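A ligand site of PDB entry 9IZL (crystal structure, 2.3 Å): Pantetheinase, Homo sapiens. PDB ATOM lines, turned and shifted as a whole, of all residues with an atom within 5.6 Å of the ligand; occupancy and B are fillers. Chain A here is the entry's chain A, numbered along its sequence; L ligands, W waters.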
ATOM      1  N   GLU A  58     -16.651   7.997  -8.104  1.00  0.00           N
ATOM      2  CA  GLU A  58     -17.137   7.865  -6.740  1.00  0.00           C
ATOM      3  C   GLU A  58     -15.950   7.752  -5.799  1.00  0.00           C
ATOM      4  O   GLU A  58     -14.920   7.194  -6.154  1.00  0.00           O
ATOM      5  CB  GLU A  58     -18.056   6.631  -6.613  1.00  0.00           C
ATOM      6  CG  GLU A  58     -18.478   6.290  -5.191  1.00  0.00           C
ATOM      7  CD  GLU A  58     -19.196   4.935  -5.091  1.00  0.00           C
ATOM      8  OE1 GLU A  58     -18.954   4.064  -5.966  1.00  0.00           O
ATOM      9  OE2 GLU A  58     -19.994   4.743  -4.145  1.00  0.00           O
ATOM     10  N   ASP A  59     -16.072   8.363  -4.611  1.00  0.00           N
ATOM     11  CA  ASP A  59     -15.010   8.325  -3.601  1.00  0.00           C
ATOM     12  C   ASP A  59     -13.721   8.960  -4.093  1.00  0.00           C
ATOM     13  O   ASP A  59     -12.648   8.793  -3.471  1.00  0.00           O
ATOM     14  CB  ASP A  59     -14.732   6.875  -3.131  1.00  0.00           C
ATOM     15  CG  ASP A  59     -15.826   6.306  -2.227  1.00  0.00           C
ATOM     16  OD1 ASP A  59     -16.594   7.060  -1.609  1.00  0.00           O
ATOM     17  OD2 ASP A  59     -15.905   5.059  -2.133  1.00  0.00           O
ATOM     18  N   TRP A  64     -12.051   5.322   0.169  1.00  0.00           N
ATOM     19  CA  TRP A  64     -13.087   4.403   0.575  1.00  0.00           C
ATOM     20  C   TRP A  64     -12.789   3.668   1.874  1.00  0.00           C
ATOM     21  O   TRP A  64     -13.584   2.798   2.270  1.00  0.00           O
ATOM     22  CB  TRP A  64     -13.345   3.388  -0.549  1.00  0.00           C
ATOM     23  CG  TRP A  64     -12.089   2.747  -0.984  1.00  0.00           C
ATOM     24  CD1 TRP A  64     -11.453   1.725  -0.360  1.00  0.00           C
ATOM     25  CD2 TRP A  64     -11.289   3.088  -2.119  1.00  0.00           C
ATOM     26  NE1 TRP A  64     -10.303   1.407  -1.028  1.00  0.00           N
ATOM     27  CE2 TRP A  64     -10.188   2.228  -2.122  1.00  0.00           C
ATOM     28  CE3 TRP A  64     -11.415   4.042  -3.138  1.00  0.00           C
ATOM     29  CZ2 TRP A  64      -9.189   2.279  -3.102  1.00  0.00           C
ATOM     30  CZ3 TRP A  64     -10.417   4.081  -4.126  1.00  0.00           C
ATOM     31  CH2 TRP A  64      -9.314   3.217  -4.078  1.00  0.00           C
ATOM     32  N   ASN A 140     -23.259   8.987   1.086  1.00  0.00           N
ATOM     33  CA  ASN A 140     -22.431   8.947  -0.121  1.00  0.00           C
ATOM     34  C   ASN A 140     -23.165   9.760  -1.188  1.00  0.00           C
ATOM     35  O   ASN A 140     -24.250   9.377  -1.641  1.00  0.00           O
ATOM     36  CB  ASN A 140     -22.215   7.483  -0.516  1.00  0.00           C
ATOM     37  CG  ASN A 140     -21.474   7.295  -1.847  1.00  0.00           C
ATOM     38  OD1 ASN A 140     -21.881   7.808  -2.870  1.00  0.00           O
ATOM     39  ND2 ASN A 140     -20.383   6.551  -1.804  1.00  0.00           N
ATOM     40  N   LYS A 157     -26.555   8.055  -2.245  1.00  0.00           N
ATOM     41  CA  LYS A 157     -26.511   6.702  -2.794  1.00  0.00           C
ATOM     42  C   LYS A 157     -27.502   5.798  -2.069  1.00  0.00           C
ATOM     43  O   LYS A 157     -27.442   5.665  -0.839  1.00  0.00           O
ATOM     44  CB  LYS A 157     -25.098   6.139  -2.675  1.00  0.00           C
ATOM     45  CG  LYS A 157     -24.888   4.764  -3.321  1.00  0.00           C
ATOM     46  CD  LYS A 157     -23.464   4.262  -3.131  1.00  0.00           C
ATOM     47  CE  LYS A 157     -23.238   2.955  -3.895  1.00  0.00           C
ATOM     48  NZ  LYS A 157     -21.853   2.391  -3.676  1.00  0.00           N
ATOM     49  N   PHE A 161     -22.930  -0.692  -1.137  1.00  0.00           N
ATOM     50  CA  PHE A 161     -22.158  -1.899  -1.314  1.00  0.00           C
ATOM     51  C   PHE A 161     -21.577  -2.319   0.039  1.00  0.00           C
ATOM     52  O   PHE A 161     -21.488  -1.521   0.975  1.00  0.00           O
ATOM     53  CB  PHE A 161     -21.057  -1.682  -2.363  1.00  0.00           C
ATOM     54  CG  PHE A 161     -20.493  -2.950  -2.908  1.00  0.00           C
ATOM     55  CD1 PHE A 161     -21.256  -3.777  -3.739  1.00  0.00           C
ATOM     56  CD2 PHE A 161     -19.216  -3.371  -2.573  1.00  0.00           C
ATOM     57  CE1 PHE A 161     -20.751  -5.003  -4.216  1.00  0.00           C
ATOM     58  CE2 PHE A 161     -18.702  -4.575  -3.044  1.00  0.00           C
ATOM     59  CZ  PHE A 161     -19.474  -5.392  -3.864  1.00  0.00           C
ATOM     60  N   MET A 162     -21.225  -3.612   0.147  1.00  0.00           N
ATOM     61  CA  MET A 162     -20.561  -4.102   1.346  1.00  0.00           C
ATOM     62  C   MET A 162     -19.268  -3.315   1.576  1.00  0.00           C
ATOM     63  O   MET A 162     -18.607  -2.865   0.632  1.00  0.00           O
ATOM     64  CB  MET A 162     -20.298  -5.613   1.259  1.00  0.00           C
ATOM     65  CG  MET A 162     -19.312  -6.071   0.204  1.00  0.00           C
ATOM     66  SD  MET A 162     -18.882  -7.852   0.317  1.00  0.00           S
ATOM     67  CE  MET A 162     -19.303  -8.280   2.011  1.00  0.00           C
ATOM     68  N   GLY A 163     -18.930  -3.105   2.847  1.00  0.00           N
ATOM     69  CA  GLY A 163     -17.784  -2.275   3.165  1.00  0.00           C
ATOM     70  C   GLY A 163     -18.067  -0.798   3.159  1.00  0.00           C
ATOM     71  O   GLY A 163     -17.128   0.004   3.291  1.00  0.00           O
ATOM     72  N   GLU A 164     -19.323  -0.394   2.988  1.00  0.00           N
ATOM     73  CA  GLU A 164     -19.723   1.003   3.103  1.00  0.00           C
ATOM     74  C   GLU A 164     -20.402   1.299   4.434  1.00  0.00           C
ATOM     75  O   GLU A 164     -21.428   1.990   4.468  1.00  0.00           O
ATOM     76  CB  GLU A 164     -20.610   1.396   1.927  1.00  0.00           C
ATOM     77  CG  GLU A 164     -19.893   1.417   0.580  1.00  0.00           C
ATOM     78  CD  GLU A 164     -20.404   2.507  -0.352  1.00  0.00           C
ATOM     79  OE1 GLU A 164     -21.423   2.277  -1.030  1.00  0.00           O
ATOM     80  OE2 GLU A 164     -19.764   3.583  -0.413  1.00  0.00           O
ATOM     81  N   THR A 189     -25.205   6.070  -8.477  1.00  0.00           N
ATOM     82  CA  THR A 189     -23.824   5.802  -8.074  1.00  0.00           C
ATOM     83  C   THR A 189     -23.521   4.306  -8.080  1.00  0.00           C
ATOM     84  O   THR A 189     -24.162   3.548  -7.342  1.00  0.00           O
ATOM     85  CB  THR A 189     -23.554   6.395  -6.681  1.00  0.00           C
ATOM     86  OG1 THR A 189     -24.106   7.716  -6.623  1.00  0.00           O
ATOM     87  CG2 THR A 189     -22.071   6.474  -6.365  1.00  0.00           C
ATOM     88  N   CYS A 190     -22.513   3.907  -8.848  1.00  0.00           N
ATOM     89  CA  CYS A 190     -21.922   2.564  -8.797  1.00  0.00           C
ATOM     90  C   CYS A 190     -22.950   1.441  -8.652  1.00  0.00           C
ATOM     91  O   CYS A 190     -23.717   1.148  -9.595  1.00  0.00           O
ATOM     92  CB  CYS A 190     -20.932   2.507  -7.623  1.00  0.00           C
ATOM     93  SG  CYS A 190     -19.490   1.434  -7.879  1.00  0.00           S
ATOM     94  N   PHE A 191     -23.012   0.852  -7.460  1.00  0.00           N
ATOM     95  CA  PHE A 191     -23.837  -0.337  -7.226  1.00  0.00           C
ATOM     96  C   PHE A 191     -25.283  -0.100  -7.651  1.00  0.00           C
ATOM     97  O   PHE A 191     -25.985  -1.055  -8.020  1.00  0.00           O
ATOM     98  CB  PHE A 191     -23.774  -0.732  -5.740  1.00  0.00           C
ATOM     99  CG  PHE A 191     -24.170  -2.176  -5.450  1.00  0.00           C
ATOM    100  CD1 PHE A 191     -24.053  -3.155  -6.415  1.00  0.00           C
ATOM    101  CD2 PHE A 191     -24.640  -2.523  -4.192  1.00  0.00           C
ATOM    102  CE1 PHE A 191     -24.403  -4.474  -6.145  1.00  0.00           C
ATOM    103  CE2 PHE A 191     -24.996  -3.839  -3.900  1.00  0.00           C
ATOM    104  CZ  PHE A 191     -24.873  -4.831  -4.885  1.00  0.00           C
ATOM    105  N   LEU A 194     -27.296  -1.826 -10.549  1.00  0.00           N
ATOM    106  CA  LEU A 194     -27.837  -3.185 -10.572  1.00  0.00           C
ATOM    107  C   LEU A 194     -29.259  -3.282 -10.039  1.00  0.00           C
ATOM    108  O   LEU A 194     -29.824  -4.385 -10.022  1.00  0.00           O
ATOM    109  CB  LEU A 194     -26.927  -4.131  -9.773  1.00  0.00           C
ATOM    110  CG  LEU A 194     -25.916  -4.858 -10.657  1.00  0.00           C
ATOM    111  CD1 LEU A 194     -24.779  -5.413  -9.793  1.00  0.00           C
ATOM    112  CD2 LEU A 194     -26.598  -5.994 -11.439  1.00  0.00           C
ATOM    113  N   ALA A 216     -16.958   3.529  -8.222  1.00  0.00           N
ATOM    114  CA  ALA A 216     -15.713   2.897  -7.754  1.00  0.00           C
ATOM    115  C   ALA A 216     -15.934   1.393  -7.879  1.00  0.00           C
ATOM    116  O   ALA A 216     -16.071   0.690  -6.870  1.00  0.00           O
ATOM    117  CB  ALA A 216     -15.386   3.320  -6.317  1.00  0.00           C
ATOM    118  N   TRP A 217     -15.828   0.889  -9.090  1.00  0.00           N
ATOM    119  CA  TRP A 217     -16.311  -0.436  -9.463  1.00  0.00           C
ATOM    120  C   TRP A 217     -15.131  -1.395  -9.521  1.00  0.00           C
ATOM    121  O   TRP A 217     -14.126  -1.099 -10.167  1.00  0.00           O
ATOM    122  CB  TRP A 217     -16.995  -0.365 -10.822  1.00  0.00           C
ATOM    123  CG  TRP A 217     -17.671  -1.590 -11.270  1.00  0.00           C
ATOM    124  CD1 TRP A 217     -17.096  -2.723 -11.807  1.00  0.00           C
ATOM    125  CD2 TRP A 217     -19.081  -1.832 -11.256  1.00  0.00           C
ATOM    126  NE1 TRP A 217     -18.061  -3.634 -12.134  1.00  0.00           N
ATOM    127  CE2 TRP A 217     -19.288  -3.123 -11.800  1.00  0.00           C
ATOM    128  CE3 TRP A 217     -20.184  -1.081 -10.831  1.00  0.00           C
ATOM    129  CZ2 TRP A 217     -20.563  -3.673 -11.945  1.00  0.00           C
ATOM    130  CZ3 TRP A 217     -21.448  -1.619 -10.971  1.00  0.00           C
ATOM    131  CH2 TRP A 217     -21.626  -2.929 -11.528  1.00  0.00           C
ATOM    132  N   MET A 218     -15.291  -2.540  -8.864  1.00  0.00           N
ATOM    133  CA  MET A 218     -14.294  -3.627  -8.872  1.00  0.00           C
ATOM    134  C   MET A 218     -14.766  -4.683  -9.868  1.00  0.00           C
ATOM    135  O   MET A 218     -15.835  -5.279  -9.691  1.00  0.00           O
ATOM    136  CB  MET A 218     -14.110  -4.222  -7.475  1.00  0.00           C
ATOM    137  CG  MET A 218     -13.514  -3.252  -6.472  1.00  0.00           C
ATOM    138  SD  MET A 218     -13.453  -3.918  -4.798  1.00  0.00           S
ATOM    139  CE  MET A 218     -15.206  -3.916  -4.444  1.00  0.00           C
ATOM    140  N   VAL A 220     -15.675  -7.787 -11.966  1.00  0.00           N
ATOM    141  CA  VAL A 220     -15.934  -9.186 -11.694  1.00  0.00           C
ATOM    142  C   VAL A 220     -16.281  -9.812 -13.033  1.00  0.00           C
ATOM    143  O   VAL A 220     -17.405  -9.678 -13.535  1.00  0.00           O
ATOM    144  CB  VAL A 220     -17.053  -9.377 -10.665  1.00  0.00           C
ATOM    145  CG1 VAL A 220     -17.225 -10.857 -10.317  1.00  0.00           C
ATOM    146  CG2 VAL A 220     -16.749  -8.545  -9.420  1.00  0.00           C
ATOM    147  N   LEU A 224     -19.444  -8.773 -15.182  1.00  0.00           N
ATOM    148  CA  LEU A 224     -19.505  -7.520 -14.437  1.00  0.00           C
ATOM    149  C   LEU A 224     -18.156  -6.807 -14.437  1.00  0.00           C
ATOM    150  O   LEU A 224     -17.691  -6.287 -13.419  1.00  0.00           O
ATOM    151  CB  LEU A 224     -20.006  -7.769 -13.011  1.00  0.00           C
ATOM    152  CG  LEU A 224     -21.395  -8.422 -12.980  1.00  0.00           C
ATOM    153  CD1 LEU A 224     -21.811  -8.866 -11.575  1.00  0.00           C
ATOM    154  CD2 LEU A 224     -22.432  -7.467 -13.576  1.00  0.00           C
ATOM    155  N   LYS A 251      -7.173  -3.311  -6.747  1.00  0.00           N
ATOM    156  CA  LYS A 251      -8.515  -3.746  -6.398  1.00  0.00           C
ATOM    157  C   LYS A 251      -9.378  -3.976  -7.629  1.00  0.00           C
ATOM    158  O   LYS A 251     -10.616  -3.974  -7.536  1.00  0.00           O
ATOM    159  CB  LYS A 251      -9.211  -2.741  -5.471  1.00  0.00           C
ATOM    160  CG  LYS A 251      -8.449  -2.369  -4.218  1.00  0.00           C
ATOM    161  CD  LYS A 251      -9.409  -1.751  -3.204  1.00  0.00           C
ATOM    162  CE  LYS A 251     -10.224  -2.850  -2.509  1.00  0.00           C
ATOM    163  NZ  LYS A 251     -11.408  -2.303  -1.766  1.00  0.00           N
ATOM    164  N   MET A 253     -10.036  -1.975  -9.983  1.00  0.00           N
ATOM    165  CA  MET A 253     -10.783  -0.756 -10.301  1.00  0.00           C
ATOM    166  C   MET A 253     -10.181  -0.161 -11.565  1.00  0.00           C
ATOM    167  O   MET A 253      -9.069   0.374 -11.546  1.00  0.00           O
ATOM    168  CB  MET A 253     -10.769   0.223  -9.138  1.00  0.00           C
ATOM    169  CG  MET A 253     -11.732  -0.144  -8.045  1.00  0.00           C
ATOM    170  SD  MET A 253     -11.442   0.868  -6.575  1.00  0.00           S
ATOM    171  CE  MET A 253     -12.745   0.271  -5.526  1.00  0.00           C
ATOM    172  N   PHE A 317     -19.576 -16.180 -10.631  1.00  0.00           N
ATOM    173  CA  PHE A 317     -19.845 -15.197  -9.569  1.00  0.00           C
ATOM    174  C   PHE A 317     -20.735 -15.787  -8.470  1.00  0.00           C
ATOM    175  O   PHE A 317     -21.671 -15.142  -7.993  1.00  0.00           O
ATOM    176  CB  PHE A 317     -20.476 -13.926 -10.160  1.00  0.00           C
ATOM    177  CG  PHE A 317     -20.422 -12.709  -9.249  1.00  0.00           C
ATOM    178  CD1 PHE A 317     -19.528 -12.632  -8.209  1.00  0.00           C
ATOM    179  CD2 PHE A 317     -21.268 -11.623  -9.472  1.00  0.00           C
ATOM    180  CE1 PHE A 317     -19.475 -11.518  -7.386  1.00  0.00           C
ATOM    181  CE2 PHE A 317     -21.219 -10.490  -8.662  1.00  0.00           C
ATOM    182  CZ  PHE A 317     -20.320 -10.441  -7.608  1.00  0.00           C
ATOM    183  N   VAL A 368     -24.526 -13.252  -3.076  1.00  0.00           N
ATOM    184  CA  VAL A 368     -23.208 -12.959  -2.506  1.00  0.00           C
ATOM    185  C   VAL A 368     -22.830 -11.527  -2.873  1.00  0.00           C
ATOM    186  O   VAL A 368     -22.703 -11.193  -4.062  1.00  0.00           O
ATOM    187  CB  VAL A 368     -22.151 -13.968  -3.006  1.00  0.00           C
ATOM    188  CG1 VAL A 368     -20.766 -13.348  -2.978  1.00  0.00           C
ATOM    189  CG2 VAL A 368     -22.172 -15.236  -2.165  1.00  0.00           C
ATOM    190  N   GLU A 369     -22.622 -10.684  -1.857  1.00  0.00           N
ATOM    191  CA  GLU A 369     -22.422  -9.248  -2.018  1.00  0.00           C
ATOM    192  C   GLU A 369     -23.484  -8.640  -2.938  1.00  0.00           C
ATOM    193  O   GLU A 369     -23.204  -8.144  -4.031  1.00  0.00           O
ATOM    194  CB  GLU A 369     -21.019  -8.918  -2.541  1.00  0.00           C
ATOM    195  CG  GLU A 369     -19.929  -9.841  -2.056  1.00  0.00           C
ATOM    196  CD  GLU A 369     -18.868  -9.995  -3.112  1.00  0.00           C
ATOM    197  OE1 GLU A 369     -18.286  -8.959  -3.516  1.00  0.00           O
ATOM    198  OE2 GLU A 369     -18.625 -11.139  -3.572  1.00  0.00           O
ATOM    199  N   TYR A 372     -30.117 -10.110  -5.753  1.00  0.00           N
ATOM    200  CA  TYR A 372     -30.883  -9.691  -6.930  1.00  0.00           C
ATOM    201  C   TYR A 372     -31.162 -10.893  -7.823  1.00  0.00           C
ATOM    202  O   TYR A 372     -30.283 -11.743  -8.016  1.00  0.00           O
ATOM    203  CB  TYR A 372     -30.163  -8.585  -7.718  1.00  0.00           C
ATOM    204  CG  TYR A 372     -28.653  -8.710  -7.760  1.00  0.00           C
ATOM    205  CD1 TYR A 372     -27.872  -8.162  -6.746  1.00  0.00           C
ATOM    206  CD2 TYR A 372     -28.003  -9.331  -8.818  1.00  0.00           C
ATOM    207  CE1 TYR A 372     -26.476  -8.259  -6.777  1.00  0.00           C
ATOM    208  CE2 TYR A 372     -26.609  -9.439  -8.857  1.00  0.00           C
ATOM    209  CZ  TYR A 372     -25.845  -8.903  -7.837  1.00  0.00           C
ATOM    210  OH  TYR A 372     -24.467  -8.979  -7.847  1.00  0.00           O
HETATM  211  C1  LIG L   1     -14.133   0.017  -2.458  1.00  0.00           C
HETATM  212  C2  LIG L   1     -16.646  -0.588  -1.589  1.00  0.00           C
HETATM  213  C3  LIG L   1     -19.308  -3.364  -7.291  1.00  0.00           C
HETATM  214  C4  LIG L   1     -17.797  -1.773  -6.279  1.00  0.00           C
HETATM  215  C5  LIG L   1     -19.934  -6.890  -8.331  1.00  0.00           C
HETATM  216  C6  LIG L   1     -21.037  -6.171  -9.207  1.00  0.00           C
HETATM  217  C7  LIG L   1     -21.015  -4.685  -8.631  1.00  0.00           C
HETATM  218  C8  LIG L   1     -19.121  -1.261  -6.006  1.00  0.00           C
HETATM  219  C9  LIG L   1     -19.339   0.093  -5.189  1.00  0.00           C
HETATM  220  C10 LIG L   1     -17.223  -0.347  -3.641  1.00  0.00           C
HETATM  221  C11 LIG L   1     -16.649   0.423  -2.676  1.00  0.00           C
HETATM  222  C12 LIG L   1     -17.855   1.347  -2.140  1.00  0.00           C
HETATM  223  C13 LIG L   1     -18.476   1.758  -3.276  1.00  0.00           C
HETATM  224  C14 LIG L   1     -15.304   0.801  -3.079  1.00  0.00           C
HETATM  225  C15 LIG L   1     -15.777  -1.776  -1.957  1.00  0.00           C
HETATM  226  C16 LIG L   1     -18.971  -5.929  -8.250  1.00  0.00           C
HETATM  227  N1  LIG L   1     -18.426   0.486  -4.160  1.00  0.00           N
HETATM  228  N2  LIG L   1     -17.938  -3.092  -7.113  1.00  0.00           N
HETATM  229  N3  LIG L   1     -19.819  -4.522  -8.014  1.00  0.00           N
HETATM  230  O1  LIG L   1     -20.221   0.838  -5.435  1.00  0.00           O
HETATM  231  O2  LIG L   1     -14.383  -1.299  -1.858  1.00  0.00           O
HETATM  232  O3  LIG L   1     -20.409  -7.229  -7.000  1.00  0.00           O
HETATM  233  S1  LIG L   1     -20.146  -2.223  -6.602  1.00  0.00           S
HETATM  234  O   HOH W   1     -17.280   4.049  -0.424  1.00  0.00           O
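OE2 of Glu 58 touches C13 of the ligand (3.5 Å). Trp 64 touches the ligand (CG to C1, 3.7 Å). Phe 161 touches the ligand. Met 162 touches the ligand. Glu 164 touches the ligand. CD1 of Leu 194 touches C6 of the ligand, at 3.9 Å. Ala 216 touches the ligand (O to C4, 3.1 Å). Trp 217 touches the ligand. CG2 of Val 220 touches C16 of the ligand, 3.6 Å away. Leu 224 touches the ligand (CD1 to C6, 3.7 Å). Met 253 touches the ligand. CZ of Phe 317 touches O3 of the ligand (3.3 Å). Hydrophobic or aromatic side chains within 4 Å of the ligand: Trp 64, Phe 161, Phe 191, Leu 194, Trp 217, Met 218, Val 220, Leu 224, Met 253 and Phe 317. Of the 24 residues printed, 17 come within 4 Å of the ligand.
Water W1 lies within hydrogen-bond range of the side-chain carboxylate of Asp 59 (2.4 Å) and the side-chain carboxylate of Glu 164 (2.5 Å).
The backbone carbonyl oxygen of Leu 224 lies within hydrogen-bond range of the indole nitrogen of Trp 217. The side-chain carboxylate of Glu 58 is in salt-bridge range of the side-chain amino group of Lys 157, 3.0 Å away. OE1 of Glu 164 is in hydrogen-bond range of N of Phe 161 (3.3 Å). The backbone NH of Ala 216 lies within hydrogen-bond range of the side-chain sulfur of Cys 190, 3.3 Å away. N of Lys 157 sits at hydrogen-bond distance from O of Asn 140 (2.7 Å). OE2 of Glu 58 lies within hydrogen-bond range of ND2 of Asn 140 (3.0 Å). OE2 of Glu 164 lies within hydrogen-bond range of ND2 of Asn 140, at 3.3 Å. The side-chain carboxylate (OE1) of Glu 58 lies within hydrogen-bond range of the backbone NH (N) of Ala 216 (3.1 Å).
The backbone NH (N) of Phe 191 sits at hydrogen-bond distance from an oxygen (O1) of the ligand. The backbone NH (N) of Met 218 lies within hydrogen-bond range of a nitrogen (N2) of the ligand (3.2 Å). An oxygen (O2) of the ligand lies within hydrogen-bond range of the side-chain amino group (NZ) of Lys 251. The side-chain amino group of Lys 157 sits at hydrogen-bond distance from an oxygen (O1) of the ligand, 2.9 Å away. SG of Cys 190 is in hydrogen-bond range of O1 of the ligand (2.6 Å).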
